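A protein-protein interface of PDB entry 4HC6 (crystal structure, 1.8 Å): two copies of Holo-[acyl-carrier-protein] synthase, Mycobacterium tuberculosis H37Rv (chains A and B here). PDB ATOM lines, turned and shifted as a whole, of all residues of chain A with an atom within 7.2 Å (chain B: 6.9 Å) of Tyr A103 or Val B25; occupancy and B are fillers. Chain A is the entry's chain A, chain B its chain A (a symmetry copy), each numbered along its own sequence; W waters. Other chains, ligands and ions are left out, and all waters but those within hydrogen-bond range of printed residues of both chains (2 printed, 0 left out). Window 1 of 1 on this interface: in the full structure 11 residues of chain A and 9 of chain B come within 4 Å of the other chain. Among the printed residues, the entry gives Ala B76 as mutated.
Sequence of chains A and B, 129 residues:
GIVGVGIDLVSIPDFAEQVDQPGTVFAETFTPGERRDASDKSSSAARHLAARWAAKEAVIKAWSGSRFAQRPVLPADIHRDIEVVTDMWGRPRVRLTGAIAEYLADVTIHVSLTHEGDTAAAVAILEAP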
ATOM      1  N   VAL A   3      -8.211   4.848  14.710  1.00  0.00           N
ATOM      2  CA  VAL A   3      -7.547   3.544  14.743  1.00  0.00           C
ATOM      3  C   VAL A   3      -6.065   3.798  15.017  1.00  0.00           C
ATOM      4  O   VAL A   3      -5.429   3.090  15.809  1.00  0.00           O
ATOM      5  CB  VAL A   3      -7.669   2.761  13.360  1.00  0.00           C
ATOM      6  CG1 VAL A   3      -6.912   1.416  13.422  1.00  0.00           C
ATOM      7  CG2 VAL A   3      -9.052   2.522  12.970  1.00  0.00           C
ATOM      8  N   TRP A  63      -0.718   2.445  11.678  1.00  0.00           N
ATOM      9  CA  TRP A  63      -1.264   1.142  11.952  1.00  0.00           C
ATOM     10  C   TRP A  63      -0.464   0.339  12.971  1.00  0.00           C
ATOM     11  O   TRP A  63      -1.047  -0.165  13.909  1.00  0.00           O
ATOM     12  CB  TRP A  63      -1.540   0.332  10.704  1.00  0.00           C
ATOM     13  CG  TRP A  63      -2.548  -0.794  11.046  1.00  0.00           C
ATOM     14  CD1 TRP A  63      -3.850  -0.652  11.425  1.00  0.00           C
ATOM     15  CD2 TRP A  63      -2.264  -2.171  11.105  1.00  0.00           C
ATOM     16  NE1 TRP A  63      -4.410  -1.886  11.687  1.00  0.00           N
ATOM     17  CE2 TRP A  63      -3.454  -2.835  11.487  1.00  0.00           C
ATOM     18  CE3 TRP A  63      -1.121  -2.924  10.862  1.00  0.00           C
ATOM     19  CZ2 TRP A  63      -3.521  -4.197  11.625  1.00  0.00           C
ATOM     20  CZ3 TRP A  63      -1.192  -4.257  11.000  1.00  0.00           C
ATOM     21  CH2 TRP A  63      -2.389  -4.894  11.386  1.00  0.00           C
ATOM     22  N   ARG A  67      -1.016  -1.227  17.742  1.00  0.00           N
ATOM     23  CA  ARG A  67      -0.859  -2.615  18.200  1.00  0.00           C
ATOM     24  C   ARG A  67       0.254  -2.730  19.228  1.00  0.00           C
ATOM     25  O   ARG A  67       1.103  -3.620  19.172  1.00  0.00           O
ATOM     26  CB  ARG A  67      -0.606  -3.544  17.001  1.00  0.00           C
ATOM     27  CG  ARG A  67      -1.591  -3.318  15.837  1.00  0.00           C
ATOM     28  CD  ARG A  67      -1.390  -4.282  14.638  1.00  0.00           C
ATOM     29  NE  ARG A  67      -1.755  -5.617  15.074  1.00  0.00           N
ATOM     30  CZ  ARG A  67      -0.916  -6.603  15.359  1.00  0.00           C
ATOM     31  NH1 ARG A  67       0.398  -6.477  15.195  1.00  0.00           N
ATOM     32  NH2 ARG A  67      -1.409  -7.746  15.789  1.00  0.00           N
ATOM     33  N   GLN A  70       2.074  -6.038  20.709  1.00  0.00           N
ATOM     34  CA  GLN A  70       1.648  -7.166  19.874  1.00  0.00           C
ATOM     35  C   GLN A  70       2.753  -7.459  18.847  1.00  0.00           C
ATOM     36  O   GLN A  70       3.394  -6.549  18.317  1.00  0.00           O
ATOM     37  CB  GLN A  70       0.291  -6.880  19.187  1.00  0.00           C
ATOM     38  CG  GLN A  70      -0.922  -6.474  20.107  1.00  0.00           C
ATOM     39  CD  GLN A  70      -2.250  -6.281  19.301  1.00  0.00           C
ATOM     40  OE1 GLN A  70      -2.749  -7.228  18.684  1.00  0.00           O
ATOM     41  NE2 GLN A  70      -2.795  -5.066  19.287  1.00  0.00           N
ATOM     42  N   ARG A  71       2.983  -8.740  18.554  1.00  0.00           N
ATOM     43  CA  ARG A  71       3.942  -9.120  17.536  1.00  0.00           C
ATOM     44  C   ARG A  71       3.562  -8.430  16.217  1.00  0.00           C
ATOM     45  O   ARG A  71       2.383  -8.419  15.827  1.00  0.00           O
ATOM     46  CB  ARG A  71       4.008 -10.657  17.363  1.00  0.00           C
ATOM     47  CG  ARG A  71       5.347 -11.159  16.827  1.00  0.00           C
ATOM     48  CD  ARG A  71       5.471 -12.702  16.841  1.00  0.00           C
ATOM     49  NE  ARG A  71       5.603 -13.248  18.188  1.00  0.00           N
ATOM     50  CZ  ARG A  71       4.592 -13.791  18.867  1.00  0.00           C
ATOM     51  NH1 ARG A  71       3.382 -13.861  18.317  1.00  0.00           N
ATOM     52  NH2 ARG A  71       4.776 -14.249  20.084  1.00  0.00           N
ATOM     53  N   VAL A  73       2.676  -7.680  12.444  1.00  0.00           N
ATOM     54  CA  VAL A  73       2.080  -8.446  11.370  1.00  0.00           C
ATOM     55  C   VAL A  73       2.225  -7.745  10.024  1.00  0.00           C
ATOM     56  O   VAL A  73       1.600  -8.158   9.042  1.00  0.00           O
ATOM     57  CB  VAL A  73       0.575  -8.717  11.632  1.00  0.00           C
ATOM     58  CG1 VAL A  73       0.413  -9.452  12.940  1.00  0.00           C
ATOM     59  CG2 VAL A  73      -0.240  -7.426  11.611  1.00  0.00           C
ATOM     60  N   LEU A  74       3.040  -6.706   9.940  1.00  0.00           N
ATOM     61  CA  LEU A  74       3.232  -6.091   8.616  1.00  0.00           C
ATOM     62  C   LEU A  74       4.239  -6.904   7.797  1.00  0.00           C
ATOM     63  O   LEU A  74       5.305  -7.294   8.294  1.00  0.00           O
ATOM     64  CB  LEU A  74       3.615  -4.631   8.712  1.00  0.00           C
ATOM     65  CG  LEU A  74       2.446  -3.683   9.091  1.00  0.00           C
ATOM     66  CD1 LEU A  74       2.955  -2.250   9.126  1.00  0.00           C
ATOM     67  CD2 LEU A  74       1.205  -3.793   8.158  1.00  0.00           C
ATOM     68  N   PRO A  75       3.901  -7.193   6.538  1.00  0.00           N
ATOM     69  CA  PRO A  75       4.841  -7.984   5.754  1.00  0.00           C
ATOM     70  C   PRO A  75       6.143  -7.217   5.474  1.00  0.00           C
ATOM     71  O   PRO A  75       6.180  -5.993   5.517  1.00  0.00           O
ATOM     72  CB  PRO A  75       4.089  -8.247   4.458  1.00  0.00           C
ATOM     73  CG  PRO A  75       3.194  -7.071   4.297  1.00  0.00           C
ATOM     74  CD  PRO A  75       2.751  -6.749   5.738  1.00  0.00           C
ATOM     75  N   LEU A  96      -3.933   0.579  -1.116  1.00  0.00           N
ATOM     76  CA  LEU A  96      -3.319  -0.577  -0.469  1.00  0.00           C
ATOM     77  C   LEU A  96      -3.461  -1.868  -1.229  1.00  0.00           C
ATOM     78  O   LEU A  96      -4.472  -2.075  -1.906  1.00  0.00           O
ATOM     79  CB  LEU A  96      -3.986  -0.818   0.876  1.00  0.00           C
ATOM     80  CG  LEU A  96      -3.949   0.336   1.848  1.00  0.00           C
ATOM     81  CD1 LEU A  96      -4.639  -0.086   3.117  1.00  0.00           C
ATOM     82  CD2 LEU A  96      -2.511   0.767   2.113  1.00  0.00           C
ATOM     83  N   GLY A  98      -2.278  -6.387  -0.736  1.00  0.00           N
ATOM     84  CA  GLY A  98      -1.785  -7.383   0.219  1.00  0.00           C
ATOM     85  C   GLY A  98      -2.557  -7.371   1.531  1.00  0.00           C
ATOM     86  O   GLY A  98      -3.681  -6.837   1.616  1.00  0.00           O
ATOM     87  N   ALA A  99      -1.950  -7.971   2.562  1.00  0.00           N
ATOM     88  CA  ALA A  99      -2.629  -8.182   3.824  1.00  0.00           C
ATOM     89  C   ALA A  99      -3.100  -6.858   4.418  1.00  0.00           C
ATOM     90  O   ALA A  99      -4.142  -6.787   5.041  1.00  0.00           O
ATOM     91  CB  ALA A  99      -1.743  -8.963   4.833  1.00  0.00           C
ATOM     92  N   ILE A 100      -2.363  -5.785   4.186  1.00  0.00           N
ATOM     93  CA  ILE A 100      -2.709  -4.531   4.864  1.00  0.00           C
ATOM     94  C   ILE A 100      -4.017  -3.988   4.304  1.00  0.00           C
ATOM     95  O   ILE A 100      -4.776  -3.351   5.010  1.00  0.00           O
ATOM     96  CB  ILE A 100      -1.591  -3.475   4.797  1.00  0.00           C
ATOM     97  CG1 ILE A 100      -1.883  -2.377   5.847  1.00  0.00           C
ATOM     98  CG2 ILE A 100      -1.426  -2.938   3.363  1.00  0.00           C
ATOM     99  CD1 ILE A 100      -0.923  -1.166   5.835  1.00  0.00           C
ATOM    100  N   ALA A 101      -4.293  -4.271   3.037  1.00  0.00           N
ATOM    101  CA  ALA A 101      -5.567  -3.911   2.434  1.00  0.00           C
ATOM    102  C   ALA A 101      -6.739  -4.615   3.145  1.00  0.00           C
ATOM    103  O   ALA A 101      -7.828  -4.035   3.310  1.00  0.00           O
ATOM    104  CB  ALA A 101      -5.554  -4.276   0.951  1.00  0.00           C
ATOM    105  N   GLU A 102      -6.526  -5.863   3.545  1.00  0.00           N
ATOM    106  CA  GLU A 102      -7.534  -6.604   4.262  1.00  0.00           C
ATOM    107  C   GLU A 102      -7.639  -6.106   5.685  1.00  0.00           C
ATOM    108  O   GLU A 102      -8.727  -5.910   6.208  1.00  0.00           O
ATOM    109  CB  GLU A 102      -7.249  -8.118   4.192  1.00  0.00           C
ATOM    110  CG  GLU A 102      -7.288  -8.645   2.732  1.00  0.00           C
ATOM    111  CD  GLU A 102      -6.987 -10.128   2.572  1.00  0.00           C
ATOM    112  OE1 GLU A 102      -7.145 -10.894   3.542  1.00  0.00           O
ATOM    113  OE2 GLU A 102      -6.615 -10.547   1.448  1.00  0.00           O
ATOM    114  N   TYR A 103      -6.513  -5.858   6.329  1.00  0.00           N
ATOM    115  CA  TYR A 103      -6.560  -5.330   7.692  1.00  0.00           C
ATOM    116  C   TYR A 103      -7.258  -3.983   7.770  1.00  0.00           C
ATOM    117  O   TYR A 103      -7.991  -3.685   8.730  1.00  0.00           O
ATOM    118  CB  TYR A 103      -5.150  -5.180   8.242  1.00  0.00           C
ATOM    119  CG  TYR A 103      -4.305  -6.450   8.330  1.00  0.00           C
ATOM    120  CD1 TYR A 103      -4.880  -7.701   8.513  1.00  0.00           C
ATOM    121  CD2 TYR A 103      -2.912  -6.375   8.302  1.00  0.00           C
ATOM    122  CE1 TYR A 103      -4.089  -8.842   8.618  1.00  0.00           C
ATOM    123  CE2 TYR A 103      -2.103  -7.523   8.420  1.00  0.00           C
ATOM    124  CZ  TYR A 103      -2.698  -8.751   8.581  1.00  0.00           C
ATOM    125  OH  TYR A 103      -1.922  -9.902   8.675  1.00  0.00           O
ATOM    126  N   LEU A 104      -7.013  -3.141   6.774  1.00  0.00           N
ATOM    127  CA  LEU A 104      -7.573  -1.803   6.776  1.00  0.00           C
ATOM    128  C   LEU A 104      -8.816  -1.707   5.874  1.00  0.00           C
ATOM    129  O   LEU A 104      -9.212  -0.613   5.489  1.00  0.00           O
ATOM    130  CB  LEU A 104      -6.482  -0.769   6.392  1.00  0.00           C
ATOM    131  CG  LEU A 104      -5.360  -0.582   7.427  1.00  0.00           C
ATOM    132  CD1 LEU A 104      -4.326   0.414   6.961  1.00  0.00           C
ATOM    133  CD2 LEU A 104      -5.955  -0.097   8.748  1.00  0.00           C
ATOM    134  N   ALA A 105      -9.474  -2.832   5.603  1.00  0.00           N
ATOM    135  CA  ALA A 105     -10.745  -2.773   4.918  1.00  0.00           C
ATOM    136  C   ALA A 105     -11.688  -2.108   5.928  1.00  0.00           C
ATOM    137  O   ALA A 105     -11.607  -2.348   7.141  1.00  0.00           O
ATOM    138  CB  ALA A 105     -11.216  -4.187   4.529  1.00  0.00           C
ATOM    139  N   ASP A 106     -12.523  -1.213   5.464  1.00  0.00           N
ATOM    140  CA  ASP A 106     -13.433  -0.488   6.370  1.00  0.00           C
ATOM    141  C   ASP A 106     -12.749   0.592   7.211  1.00  0.00           C
ATOM    142  O   ASP A 106     -13.380   1.104   8.149  1.00  0.00           O
ATOM    143  CB  ASP A 106     -14.184  -1.430   7.338  1.00  0.00           C
ATOM    144  N   VAL A 107     -11.485   0.916   6.917  1.00  0.00           N
ATOM    145  CA  VAL A 107     -10.815   2.022   7.598  1.00  0.00           C
ATOM    146  C   VAL A 107     -10.515   3.081   6.545  1.00  0.00           C
ATOM    147  O   VAL A 107     -10.010   2.757   5.422  1.00  0.00           O
ATOM    148  CB  VAL A 107      -9.501   1.584   8.263  1.00  0.00           C
ATOM    149  CG1 VAL A 107      -8.683   2.819   8.816  1.00  0.00           C
ATOM    150  CG2 VAL A 107      -9.753   0.501   9.347  1.00  0.00           C
ATOM    151  N   VAL B  19     -12.408  -7.886  18.515  1.00  0.00           N
ATOM    152  CA  VAL B  19     -12.514  -8.934  17.507  1.00  0.00           C
ATOM    153  C   VAL B  19     -13.314  -8.509  16.272  1.00  0.00           C
ATOM    154  O   VAL B  19     -12.975  -8.908  15.159  1.00  0.00           O
ATOM    155  CB  VAL B  19     -13.041 -10.263  18.099  1.00  0.00           C
ATOM    156  CG1 VAL B  19     -14.522 -10.134  18.423  1.00  0.00           C
ATOM    157  CG2 VAL B  19     -12.770 -11.408  17.151  1.00  0.00           C
ATOM    158  N   GLN B  21     -13.720  -5.241  15.282  1.00  0.00           N
ATOM    159  CA  GLN B  21     -13.423  -3.844  14.946  1.00  0.00           C
ATOM    160  C   GLN B  21     -12.647  -3.807  13.662  1.00  0.00           C
ATOM    161  O   GLN B  21     -11.766  -4.647  13.426  1.00  0.00           O
ATOM    162  CB  GLN B  21     -12.655  -3.130  16.068  1.00  0.00           C
ATOM    163  CG  GLN B  21     -13.452  -3.000  17.383  1.00  0.00           C
ATOM    164  CD  GLN B  21     -14.951  -2.563  17.192  1.00  0.00           C
ATOM    165  OE1 GLN B  21     -15.260  -1.615  16.452  1.00  0.00           O
ATOM    166  NE2 GLN B  21     -15.873  -3.274  17.872  1.00  0.00           N
ATOM    167  N   PRO B  22     -12.960  -2.822  12.807  1.00  0.00           N
ATOM    168  CA  PRO B  22     -12.122  -2.664  11.633  1.00  0.00           C
ATOM    169  C   PRO B  22     -10.714  -2.264  12.048  1.00  0.00           C
ATOM    170  O   PRO B  22     -10.528  -1.750  13.156  1.00  0.00           O
ATOM    171  CB  PRO B  22     -12.806  -1.528  10.847  1.00  0.00           C
ATOM    172  CG  PRO B  22     -14.156  -1.389  11.433  1.00  0.00           C
ATOM    173  CD  PRO B  22     -14.040  -1.822  12.859  1.00  0.00           C
ATOM    174  N   GLY B  23      -9.741  -2.530  11.181  1.00  0.00           N
ATOM    175  CA  GLY B  23      -8.345  -2.222  11.475  1.00  0.00           C
ATOM    176  C   GLY B  23      -7.664  -3.183  12.445  1.00  0.00           C
ATOM    177  O   GLY B  23      -6.780  -2.776  13.226  1.00  0.00           O
ATOM    178  N   THR B  24      -8.054  -4.454  12.389  1.00  0.00           N
ATOM    179  CA  THR B  24      -7.453  -5.501  13.231  1.00  0.00           C
ATOM    180  C   THR B  24      -7.119  -6.719  12.341  1.00  0.00           C
ATOM    181  O   THR B  24      -7.605  -6.822  11.216  1.00  0.00           O
ATOM    182  CB  THR B  24      -8.445  -5.940  14.320  1.00  0.00           C
ATOM    183  OG1 THR B  24      -9.603  -6.509  13.704  1.00  0.00           O
ATOM    184  CG2 THR B  24      -8.881  -4.764  15.191  1.00  0.00           C
ATOM    185  N   VAL B  25      -6.301  -7.639  12.834  1.00  0.00           N
ATOM    186  CA  VAL B  25      -5.986  -8.837  12.045  1.00  0.00           C
ATOM    187  C   VAL B  25      -7.096  -9.874  11.952  1.00  0.00           C
ATOM    188  O   VAL B  25      -7.011 -10.822  11.154  1.00  0.00           O
ATOM    189  CB  VAL B  25      -4.719  -9.504  12.572  1.00  0.00           C
ATOM    190  CG1 VAL B  25      -3.547  -8.568  12.314  1.00  0.00           C
ATOM    191  CG2 VAL B  25      -4.854  -9.835  14.047  1.00  0.00           C
ATOM    192  N   PHE B  26      -8.153  -9.684  12.737  1.00  0.00           N
ATOM    193  CA  PHE B  26      -9.136 -10.727  13.000  1.00  0.00           C
ATOM    194  C   PHE B  26     -10.011 -11.223  11.844  1.00  0.00           C
ATOM    195  O   PHE B  26     -10.452 -12.368  11.864  1.00  0.00           O
ATOM    196  CB  PHE B  26     -10.000 -10.281  14.177  1.00  0.00           C
ATOM    197  CG  PHE B  26      -9.230 -10.173  15.464  1.00  0.00           C
ATOM    198  CD1 PHE B  26      -8.557 -11.271  15.968  1.00  0.00           C
ATOM    199  CD2 PHE B  26      -9.149  -8.991  16.158  1.00  0.00           C
ATOM    200  CE1 PHE B  26      -7.842 -11.184  17.142  1.00  0.00           C
ATOM    201  CE2 PHE B  26      -8.437  -8.903  17.342  1.00  0.00           C
ATOM    202  CZ  PHE B  26      -7.787 -10.014  17.841  1.00  0.00           C
ATOM    203  N   ALA B  27     -10.247 -10.399  10.841  1.00  0.00           N
ATOM    204  CA  ALA B  27     -11.019 -10.836   9.661  1.00  0.00           C
ATOM    205  C   ALA B  27     -10.351 -12.007   8.918  1.00  0.00           C
ATOM    206  O   ALA B  27     -11.035 -12.820   8.253  1.00  0.00           O
ATOM    207  CB  ALA B  27     -11.229  -9.672   8.718  1.00  0.00           C
ATOM    208  N   GLU B  28      -9.024 -12.084   9.056  1.00  0.00           N
ATOM    209  CA  GLU B  28      -8.203 -13.074   8.362  1.00  0.00           C
ATOM    210  C   GLU B  28      -8.276 -14.423   9.028  1.00  0.00           C
ATOM    211  O   GLU B  28      -7.999 -15.456   8.413  1.00  0.00           O
ATOM    212  CB  GLU B  28      -6.749 -12.613   8.331  1.00  0.00           C
ATOM    213  CG  GLU B  28      -6.559 -11.296   7.627  1.00  0.00           C
ATOM    214  CD  GLU B  28      -7.173 -11.342   6.262  1.00  0.00           C
ATOM    215  OE1 GLU B  28      -8.195 -10.640   6.030  1.00  0.00           O
ATOM    216  OE2 GLU B  28      -6.672 -12.146   5.437  1.00  0.00           O
ATOM    217  N   THR B  29      -8.652 -14.416  10.294  1.00  0.00           N
ATOM    218  CA  THR B  29      -8.726 -15.631  11.052  1.00  0.00           C
ATOM    219  C   THR B  29     -10.194 -16.074  11.219  1.00  0.00           C
ATOM    220  O   THR B  29     -10.505 -17.261  11.083  1.00  0.00           O
ATOM    221  CB  THR B  29      -7.926 -15.456  12.409  1.00  0.00           C
ATOM    222  OG1 THR B  29      -8.059 -14.111  12.886  1.00  0.00           O
ATOM    223  CG2 THR B  29      -6.446 -15.685  12.187  1.00  0.00           C
ATOM    224  N   PHE B  30     -11.107 -15.118  11.424  1.00  0.00           N
ATOM    225  CA  PHE B  30     -12.454 -15.445  11.828  1.00  0.00           C
ATOM    226  C   PHE B  30     -13.507 -14.937  10.842  1.00  0.00           C
ATOM    227  O   PHE B  30     -13.320 -13.894  10.219  1.00  0.00           O
ATOM    228  CB  PHE B  30     -12.708 -14.851  13.213  1.00  0.00           C
ATOM    229  CG  PHE B  30     -11.761 -15.358  14.278  1.00  0.00           C
ATOM    230  CD1 PHE B  30     -11.591 -16.722  14.483  1.00  0.00           C
ATOM    231  CD2 PHE B  30     -11.071 -14.473  15.091  1.00  0.00           C
ATOM    232  CE1 PHE B  30     -10.741 -17.191  15.481  1.00  0.00           C
ATOM    233  CE2 PHE B  30     -10.214 -14.930  16.084  1.00  0.00           C
ATOM    234  CZ  PHE B  30     -10.041 -16.296  16.276  1.00  0.00           C
ATOM    235  N   ARG B  35     -16.986 -13.268  14.283  1.00  0.00           N
ATOM    236  CA  ARG B  35     -16.551 -11.968  14.820  1.00  0.00           C
ATOM    237  C   ARG B  35     -17.702 -11.184  15.455  1.00  0.00           C
ATOM    238  O   ARG B  35     -17.551 -10.650  16.546  1.00  0.00           O
ATOM    239  CB  ARG B  35     -15.867 -11.146  13.740  1.00  0.00           C
ATOM    240  CG  ARG B  35     -14.525 -11.691  13.248  1.00  0.00           C
ATOM    241  CD  ARG B  35     -13.986 -10.799  12.140  1.00  0.00           C
ATOM    242  NE  ARG B  35     -13.454  -9.517  12.627  1.00  0.00           N
ATOM    243  CZ  ARG B  35     -13.379  -8.378  11.925  1.00  0.00           C
ATOM    244  NH1 ARG B  35     -13.809  -8.303  10.654  1.00  0.00           N
ATOM    245  NH2 ARG B  35     -12.856  -7.287  12.500  1.00  0.00           N
ATOM    246  N   TRP B  53      -7.782 -18.071  19.824  1.00  0.00           N
ATOM    247  CA  TRP B  53      -6.725 -17.083  19.655  1.00  0.00           C
ATOM    248  C   TRP B  53      -5.524 -17.424  20.584  1.00  0.00           C
ATOM    249  O   TRP B  53      -4.354 -17.425  20.156  1.00  0.00           O
ATOM    250  CB  TRP B  53      -7.234 -15.642  19.912  1.00  0.00           C
ATOM    251  CG  TRP B  53      -6.220 -14.639  19.526  1.00  0.00           C
ATOM    252  CD1 TRP B  53      -5.376 -13.926  20.343  1.00  0.00           C
ATOM    253  CD2 TRP B  53      -5.884 -14.281  18.189  1.00  0.00           C
ATOM    254  NE1 TRP B  53      -4.551 -13.126  19.575  1.00  0.00           N
ATOM    255  CE2 TRP B  53      -4.852 -13.327  18.250  1.00  0.00           C
ATOM    256  CE3 TRP B  53      -6.401 -14.640  16.949  1.00  0.00           C
ATOM    257  CZ2 TRP B  53      -4.308 -12.739  17.100  1.00  0.00           C
ATOM    258  CZ3 TRP B  53      -5.842 -14.071  15.807  1.00  0.00           C
ATOM    259  CH2 TRP B  53      -4.818 -13.137  15.895  1.00  0.00           C
ATOM    260  N   ALA B  76       4.770 -12.697   8.568  1.00  0.00           N
ATOM    261  CA  ALA B  76       3.928 -11.669   9.141  1.00  0.00           C
ATOM    262  C   ALA B  76       2.467 -12.137   9.324  1.00  0.00           C
ATOM    263  O   ALA B  76       1.860 -11.806  10.332  1.00  0.00           O
ATOM    264  CB  ALA B  76       3.999 -10.405   8.247  1.00  0.00           C
ATOM    265  N   ASP B  77       1.935 -12.935   8.392  1.00  0.00           N
ATOM    266  CA  ASP B  77       0.560 -13.448   8.447  1.00  0.00           C
ATOM    267  C   ASP B  77       0.428 -14.821   9.147  1.00  0.00           C
ATOM    268  O   ASP B  77      -0.490 -15.566   8.899  1.00  0.00           O
ATOM    269  CB  ASP B  77      -0.070 -13.537   7.045  1.00  0.00           C
ATOM    270  CG  ASP B  77       0.549 -14.635   6.152  1.00  0.00           C
ATOM    271  OD1 ASP B  77       1.667 -15.094   6.438  1.00  0.00           O
ATOM    272  OD2 ASP B  77      -0.110 -15.025   5.149  1.00  0.00           O
ATOM    273  N   ILE B  78       1.335 -15.093  10.069  1.00  0.00           N
ATOM    274  CA  ILE B  78       1.363 -16.357  10.783  1.00  0.00           C
ATOM    275  C   ILE B  78       0.043 -16.686  11.468  1.00  0.00           C
ATOM    276  O   ILE B  78      -0.354 -17.855  11.518  1.00  0.00           O
ATOM    277  CB  ILE B  78       2.524 -16.349  11.813  1.00  0.00           C
ATOM    278  CG1 ILE B  78       2.691 -17.724  12.487  1.00  0.00           C
ATOM    279  CG2 ILE B  78       2.362 -15.171  12.812  1.00  0.00           C
ATOM    280  CD1 ILE B  78       2.824 -18.893  11.486  1.00  0.00           C
ATOM    281  N   HIS B  79      -0.668 -15.674  11.975  1.00  0.00           N
ATOM    282  CA  HIS B  79      -1.951 -15.955  12.675  1.00  0.00           C
ATOM    283  C   HIS B  79      -2.956 -16.634  11.791  1.00  0.00           C
ATOM    284  O   HIS B  79      -3.722 -17.491  12.259  1.00  0.00           O
ATOM    285  CB  HIS B  79      -2.548 -14.715  13.318  1.00  0.00           C
ATOM    286  CG  HIS B  79      -1.690 -14.152  14.392  1.00  0.00           C
ATOM    287  ND1 HIS B  79      -0.674 -13.256  14.137  1.00  0.00           N
ATOM    288  CD2 HIS B  79      -1.644 -14.419  15.717  1.00  0.00           C
ATOM    289  CE1 HIS B  79      -0.049 -12.987  15.272  1.00  0.00           C
ATOM    290  NE2 HIS B  79      -0.623 -13.674  16.242  1.00  0.00           N
ATOM    291  N   ARG B  80      -2.978 -16.316  10.509  1.00  0.00           N
ATOM    292  CA  ARG B  80      -3.932 -16.987   9.633  1.00  0.00           C
ATOM    293  C   ARG B  80      -3.411 -18.315   9.078  1.00  0.00           C
ATOM    294  O   ARG B  80      -4.168 -19.047   8.428  1.00  0.00           O
ATOM    295  CB  ARG B  80      -4.393 -16.055   8.507  1.00  0.00           C
ATOM    296  CG  ARG B  80      -3.371 -15.756   7.456  1.00  0.00           C
ATOM    297  CD  ARG B  80      -3.942 -14.686   6.485  1.00  0.00           C
ATOM    298  NE  ARG B  80      -2.992 -14.313   5.448  1.00  0.00           N
ATOM    299  CZ  ARG B  80      -3.197 -13.391   4.505  1.00  0.00           C
ATOM    300  NH1 ARG B  80      -4.323 -12.689   4.447  1.00  0.00           N
ATOM    301  NH2 ARG B  80      -2.241 -13.154   3.618  1.00  0.00           N
HETATM  302  O   HOH W   1       0.461  -9.958   7.419  1.00  0.00           O
HETATM  303  O   HOH W   2      -3.470 -11.095   1.380  1.00  0.00           O
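Among the printed residues, pairs that only touch across the chains: Leu A74 with Ala B76 (3.4 Å), Val A73 with Ala B76 (3.4 Å), Val A107 with Gly B23 (3.5 Å), Val A73 with Val B25 (3.6 Å), Pro A75 with Ala B76 (3.6 Å), Tyr A103 with Glu B28 (3.6 Å), Tyr A103 with Thr B24 (3.7 Å), Tyr A103 with Val B25 (3.7 Å), Asp A106 with Pro B22 (3.8 Å), Val A107 with Pro B22 (3.96 Å), Trp A63 with Val B25 (3.96 Å) and Ala A105 with Pro B22 (3.98 Å).
NE of Arg B80 lies within salt-bridge range of OD2 of Asp B77 (3.0 Å).
The side-chain hydroxyl of Thr B24 lies within hydrogen-bond range of the backbone carbonyl oxygen of Gln B21 (2.9 Å).
The guanidinium group (NH1) of Arg B80 lies within salt-bridge range of the side-chain carboxylate (OE2) of Glu B28 (2.6 Å).
No position is printed for both chains.
Of the 16 pairs that touch across the chains among the printed residues, none has its exchanged pair printed and touching as well.
Printed residues of chain B that touch a printed residue of chain A: Pro B22, Gly B23, Thr B24, Val B25, Glu B28, Ala B76 and Arg B80.
Hydrophobic or aromatic side chains of chain A within 4 Å of the printed part of chain B: Trp A63, Val A73, Tyr A103 and Val A107.
Among the printed residues, Asp or Glu carboxylates within 4 Å of a Lys or Arg side-chain nitrogen of the other chain: Glu A102 with Arg B80 (3.5 Å).
Of the printed residues of chain B, Tyr A103 touches Gly B23, Thr B24, Val B25 and Glu B28.
Val B25 touches three residues of chain A.
Of the printed residues of chain A, Glu B28 touches Glu A102 and Tyr A103.
Printed residues of chain A within 4 Å of Arg B80: Glu A102.
Of the printed residues of chain B, Val A73 touches Val B25 (3.6 Å) and Ala B76 (3.4 Å).
Val B19 touches none of the printed residues of chain A.
Gln B21 touches none of the printed residues of chain A.
The nearest printed residue of chain B that does not touch Leu A74 is Asp B77 (6.5 Å).
Water W1 lies within hydrogen-bond range of O of Val A73, OH of Tyr A103 and N of Asp B77.
Water W2 lies within hydrogen-bond range of OE2 of Glu A102 (3.2 Å) and NH2 of Arg B80 (3.3 Å).
The side-chain carboxylate (OE1) of Glu A102 is in salt-bridge range of the guanidinium group (NH1) of Arg B80 (3.5 Å).
OE1 of Glu A102 sits close to OE1 of Glu B28.
N of Gly B23 sits close to O of Tyr A103.
The indole nitrogen of Trp A63 sits at hydrogen-bond distance from the backbone carbonyl oxygen of Gly B23 (3.0 Å).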
